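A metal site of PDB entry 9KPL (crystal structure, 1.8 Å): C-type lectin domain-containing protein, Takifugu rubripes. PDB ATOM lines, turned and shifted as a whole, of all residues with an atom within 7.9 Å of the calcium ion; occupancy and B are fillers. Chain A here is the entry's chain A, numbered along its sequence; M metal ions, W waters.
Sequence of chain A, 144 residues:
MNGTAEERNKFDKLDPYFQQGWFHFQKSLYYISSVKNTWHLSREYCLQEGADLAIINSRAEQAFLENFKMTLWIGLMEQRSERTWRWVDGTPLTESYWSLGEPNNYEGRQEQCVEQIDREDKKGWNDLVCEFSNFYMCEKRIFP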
ATOM      1  N   PHE A  25     -22.886 -11.731 -18.151  1.00  0.00           N
ATOM      2  CA  PHE A  25     -21.665 -11.064 -18.568  1.00  0.00           C
ATOM      3  C   PHE A  25     -20.581 -11.366 -17.534  1.00  0.00           C
ATOM      4  O   PHE A  25     -20.784 -11.092 -16.367  1.00  0.00           O
ATOM      5  CB  PHE A  25     -21.950  -9.543 -18.704  1.00  0.00           C
ATOM      6  CG  PHE A  25     -20.715  -8.723 -19.006  1.00  0.00           C
ATOM      7  CD1 PHE A  25     -20.207  -8.637 -20.317  1.00  0.00           C
ATOM      8  CD2 PHE A  25     -20.048  -8.048 -17.973  1.00  0.00           C
ATOM      9  CE1 PHE A  25     -19.043  -7.925 -20.596  1.00  0.00           C
ATOM     10  CE2 PHE A  25     -18.852  -7.336 -18.252  1.00  0.00           C
ATOM     11  CZ  PHE A  25     -18.351  -7.250 -19.576  1.00  0.00           C
ATOM     12  N   GLN A  26     -19.453 -11.959 -17.942  1.00  0.00           N
ATOM     13  CA  GLN A  26     -18.288 -12.259 -17.082  1.00  0.00           C
ATOM     14  C   GLN A  26     -18.677 -12.784 -15.692  1.00  0.00           C
ATOM     15  O   GLN A  26     -18.290 -12.225 -14.675  1.00  0.00           O
ATOM     16  CB  GLN A  26     -17.371 -11.028 -16.937  1.00  0.00           C
ATOM     17  CG  GLN A  26     -16.900 -10.452 -18.291  1.00  0.00           C
ATOM     18  CD  GLN A  26     -15.665  -9.538 -18.185  1.00  0.00           C
ATOM     19  OE1 GLN A  26     -15.598  -8.658 -17.310  1.00  0.00           O
ATOM     20  NE2 GLN A  26     -14.705  -9.706 -19.121  1.00  0.00           N
ATOM     21  N   SER A  28     -21.277 -12.871 -13.937  1.00  0.00           N
ATOM     22  CA  SER A  28     -22.487 -12.418 -13.256  1.00  0.00           C
ATOM     23  C   SER A  28     -23.699 -12.540 -14.168  1.00  0.00           C
ATOM     24  O   SER A  28     -23.572 -12.474 -15.385  1.00  0.00           O
ATOM     25  CB  SER A  28     -22.386 -10.924 -12.848  1.00  0.00           C
ATOM     26  OG  SER A  28     -21.491 -10.829 -11.715  1.00  0.00           O
ATOM     27  N   TYR A  30     -27.313 -10.312 -14.814  1.00  0.00           N
ATOM     28  CA  TYR A  30     -27.766  -8.931 -14.738  1.00  0.00           C
ATOM     29  C   TYR A  30     -29.228  -8.900 -15.128  1.00  0.00           C
ATOM     30  O   TYR A  30     -29.671  -9.731 -15.920  1.00  0.00           O
ATOM     31  CB  TYR A  30     -26.968  -7.995 -15.678  1.00  0.00           C
ATOM     32  CG  TYR A  30     -25.514  -7.916 -15.295  1.00  0.00           C
ATOM     33  CD1 TYR A  30     -24.597  -8.838 -15.772  1.00  0.00           C
ATOM     34  CD2 TYR A  30     -25.073  -6.971 -14.402  1.00  0.00           C
ATOM     35  CE1 TYR A  30     -23.230  -8.750 -15.472  1.00  0.00           C
ATOM     36  CE2 TYR A  30     -23.703  -6.842 -14.081  1.00  0.00           C
ATOM     37  CZ  TYR A  30     -22.808  -7.775 -14.586  1.00  0.00           C
ATOM     38  OH  TYR A  30     -21.470  -7.688 -14.327  1.00  0.00           O
ATOM     39  N   LEU A  53     -28.321  -4.373  -6.235  1.00  0.00           N
ATOM     40  CA  LEU A  53     -27.984  -3.445  -7.310  1.00  0.00           C
ATOM     41  C   LEU A  53     -26.563  -3.685  -7.802  1.00  0.00           C
ATOM     42  O   LEU A  53     -25.718  -4.225  -7.093  1.00  0.00           O
ATOM     43  CB  LEU A  53     -28.119  -2.004  -6.801  1.00  0.00           C
ATOM     44  CG  LEU A  53     -29.589  -1.535  -6.662  1.00  0.00           C
ATOM     45  CD1 LEU A  53     -29.526  -0.180  -5.956  1.00  0.00           C
ATOM     46  CD2 LEU A  53     -30.317  -1.391  -8.034  1.00  0.00           C
ATOM     47  N   ALA A  54     -26.311  -3.332  -9.041  1.00  0.00           N
ATOM     48  CA  ALA A  54     -25.052  -3.705  -9.678  1.00  0.00           C
ATOM     49  C   ALA A  54     -23.845  -3.001  -9.023  1.00  0.00           C
ATOM     50  O   ALA A  54     -23.930  -1.845  -8.602  1.00  0.00           O
ATOM     51  CB  ALA A  54     -25.116  -3.386 -11.170  1.00  0.00           C
ATOM     52  N   ILE A  55     -22.747  -3.736  -8.908  1.00  0.00           N
ATOM     53  CA  ILE A  55     -21.490  -3.245  -8.312  1.00  0.00           C
ATOM     54  C   ILE A  55     -20.453  -3.221  -9.441  1.00  0.00           C
ATOM     55  O   ILE A  55     -20.242  -4.268 -10.078  1.00  0.00           O
ATOM     56  CB  ILE A  55     -21.017  -4.185  -7.195  1.00  0.00           C
ATOM     57  CG1 ILE A  55     -22.040  -4.158  -6.042  1.00  0.00           C
ATOM     58  CG2 ILE A  55     -19.541  -3.734  -6.778  1.00  0.00           C
ATOM     59  CD1 ILE A  55     -21.712  -5.267  -4.968  1.00  0.00           C
ATOM     60  N   ILE A  56     -19.832  -2.081  -9.732  1.00  0.00           N
ATOM     61  CA  ILE A  56     -18.934  -1.995 -10.889  1.00  0.00           C
ATOM     62  C   ILE A  56     -17.521  -2.312 -10.420  1.00  0.00           C
ATOM     63  O   ILE A  56     -16.941  -1.583  -9.598  1.00  0.00           O
ATOM     64  CB  ILE A  56     -19.022  -0.606 -11.545  1.00  0.00           C
ATOM     65  CG1 ILE A  56     -20.461  -0.367 -11.968  1.00  0.00           C
ATOM     66  CG2 ILE A  56     -18.044  -0.533 -12.749  1.00  0.00           C
ATOM     67  CD1 ILE A  56     -21.100  -1.430 -12.902  1.00  0.00           C
ATOM     68  N   ASN A  57     -16.942  -3.430 -10.929  1.00  0.00           N
ATOM     69  CA  ASN A  57     -15.652  -3.924 -10.409  1.00  0.00           C
ATOM     70  C   ASN A  57     -14.507  -3.807 -11.421  1.00  0.00           C
ATOM     71  O   ASN A  57     -13.368  -4.084 -11.078  1.00  0.00           O
ATOM     72  CB  ASN A  57     -15.738  -5.378  -9.957  1.00  0.00           C
ATOM     73  CG  ASN A  57     -16.819  -5.615  -8.950  1.00  0.00           C
ATOM     74  OD1 ASN A  57     -17.980  -5.949  -9.298  1.00  0.00           O
ATOM     75  ND2 ASN A  57     -16.461  -5.417  -7.696  1.00  0.00           N
ATOM     76  N   SER A  58     -14.773  -3.364 -12.627  1.00  0.00           N
ATOM     77  CA  SER A  58     -13.716  -3.276 -13.626  1.00  0.00           C
ATOM     78  C   SER A  58     -14.119  -2.307 -14.731  1.00  0.00           C
ATOM     79  O   SER A  58     -15.296  -1.974 -14.899  1.00  0.00           O
ATOM     80  CB  SER A  58     -13.410  -4.634 -14.239  1.00  0.00           C
ATOM     81  OG  SER A  58     -14.491  -5.064 -15.042  1.00  0.00           O
ATOM     82  N   GLU A  61     -16.658  -3.897 -17.015  1.00  0.00           N
ATOM     83  CA  GLU A  61     -18.033  -3.897 -16.508  1.00  0.00           C
ATOM     84  C   GLU A  61     -18.662  -2.500 -16.629  1.00  0.00           C
ATOM     85  O   GLU A  61     -19.857  -2.361 -16.933  1.00  0.00           O
ATOM     86  CB  GLU A  61     -17.991  -4.367 -15.049  1.00  0.00           C
ATOM     87  CG  GLU A  61     -19.393  -4.716 -14.527  1.00  0.00           C
ATOM     88  CD  GLU A  61     -19.448  -5.307 -13.127  1.00  0.00           C
ATOM     89  OE1 GLU A  61     -18.454  -5.266 -12.349  1.00  0.00           O
ATOM     90  OE2 GLU A  61     -20.558  -5.850 -12.847  1.00  0.00           O
ATOM     91  N   TRP A  87     -20.084   0.543  -1.746  1.00  0.00           N
ATOM     92  CA  TRP A  87     -20.966  -0.293  -2.581  1.00  0.00           C
ATOM     93  C   TRP A  87     -21.957  -1.056  -1.692  1.00  0.00           C
ATOM     94  O   TRP A  87     -21.734  -1.198  -0.480  1.00  0.00           O
ATOM     95  CB  TRP A  87     -20.134  -1.275  -3.401  1.00  0.00           C
ATOM     96  CG  TRP A  87     -19.249  -0.605  -4.417  1.00  0.00           C
ATOM     97  CD1 TRP A  87     -17.865  -0.305  -4.352  1.00  0.00           C
ATOM     98  CD2 TRP A  87     -19.704  -0.171  -5.687  1.00  0.00           C
ATOM     99  NE1 TRP A  87     -17.492   0.329  -5.540  1.00  0.00           N
ATOM    100  CE2 TRP A  87     -18.578   0.387  -6.385  1.00  0.00           C
ATOM    101  CE3 TRP A  87     -20.954  -0.233  -6.329  1.00  0.00           C
ATOM    102  CZ2 TRP A  87     -18.690   0.925  -7.670  1.00  0.00           C
ATOM    103  CZ3 TRP A  87     -21.046   0.332  -7.672  1.00  0.00           C
ATOM    104  CH2 TRP A  87     -19.959   0.874  -8.288  1.00  0.00           C
ATOM    105  N   GLU A 139     -27.557  -7.223 -10.151  1.00  0.00           N
ATOM    106  CA  GLU A 139     -26.425  -8.095 -10.515  1.00  0.00           C
ATOM    107  C   GLU A 139     -26.382  -9.220  -9.472  1.00  0.00           C
ATOM    108  O   GLU A 139     -26.481  -8.947  -8.270  1.00  0.00           O
ATOM    109  CB  GLU A 139     -25.072  -7.365 -10.478  1.00  0.00           C
ATOM    110  CG  GLU A 139     -23.888  -8.337 -10.809  1.00  0.00           C
ATOM    111  CD  GLU A 139     -22.527  -7.644 -10.672  1.00  0.00           C
ATOM    112  OE1 GLU A 139     -22.425  -6.479 -10.241  1.00  0.00           O
ATOM    113  OE2 GLU A 139     -21.532  -8.263 -11.030  1.00  0.00           O
ATOM    114  N   LYS A 140     -26.184 -10.461  -9.947  1.00  0.00           N
ATOM    115  CA  LYS A 140     -26.005 -11.625  -9.090  1.00  0.00           C
ATOM    116  C   LYS A 140     -24.720 -12.293  -9.558  1.00  0.00           C
ATOM    117  O   LYS A 140     -24.606 -12.656 -10.741  1.00  0.00           O
ATOM    118  CB  LYS A 140     -27.249 -12.541  -9.262  1.00  0.00           C
ATOM    119  CG  LYS A 140     -27.217 -13.879  -8.564  1.00  0.00           C
ATOM    120  CD  LYS A 140     -28.447 -14.730  -8.871  1.00  0.00           C
ATOM    121  CE  LYS A 140     -29.738 -14.185  -8.200  1.00  0.00           C
ATOM    122  NZ  LYS A 140     -30.281 -15.181  -7.170  1.00  0.00           N
ATOM    123  N   ARG A 141     -23.698 -12.409  -8.679  1.00  0.00           N
ATOM    124  CA  ARG A 141     -22.522 -13.181  -9.043  1.00  0.00           C
ATOM    125  C   ARG A 141     -22.866 -14.657  -9.047  1.00  0.00           C
ATOM    126  O   ARG A 141     -23.460 -15.165  -8.108  1.00  0.00           O
ATOM    127  CB  ARG A 141     -21.372 -12.945  -8.040  1.00  0.00           C
ATOM    128  CG  ARG A 141     -20.998 -11.479  -8.004  1.00  0.00           C
ATOM    129  CD  ARG A 141     -19.729 -11.180  -7.165  1.00  0.00           C
ATOM    130  NE  ARG A 141     -18.569 -11.945  -7.608  1.00  0.00           N
ATOM    131  CZ  ARG A 141     -17.487 -12.146  -6.843  1.00  0.00           C
ATOM    132  NH1 ARG A 141     -17.379 -11.556  -5.658  1.00  0.00           N
ATOM    133  NH2 ARG A 141     -16.488 -12.879  -7.310  1.00  0.00           N
HETATM  134 CA    CA M   1     -19.884  -6.522 -10.574  1.00  0.00          CA
HETATM  135  O   HOH W   1     -20.111  -7.582  -8.358  1.00  0.00           O
HETATM  136  O   HOH W   2     -18.365  -8.309 -11.467  1.00  0.00           O
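The calcium ion is bound by the backbone carbonyl oxygen (O) of Ile 55 (2.3 Å), the side-chain amide oxygen (OD1) of Asn 57 (2.4 Å), the side-chain carboxylate (OE2) of Glu 139 (2.4 Å), the side-chain carboxylate (OE2) of Glu 61 (2.5 Å), water W1 (2.5 Å), water W2 (2.5 Å), the side-chain carboxylate (OE1) of Glu 139 (2.6 Å) and the side-chain carboxylate (OE1) of Glu 61 (2.6 Å).
The calcium ion has eight donor atoms within binding distance.
The nearest printed residue that does not touch the calcium ion is Tyr 30 (4.2 Å).
OE2 of Glu 139 sits close to OG of Ser 28 (2.7 Å).
OE2 of Glu 61 lies close to OH of Tyr 30, at 2.5 Å.
The side-chain hydroxyl (OH) of Tyr 30 lies close to the side-chain carboxylate (OE2) of Glu 139, at 3.3 Å.
N of Glu 61 lies within hydrogen-bond range of OG of Ser 58, 3.2 Å away.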
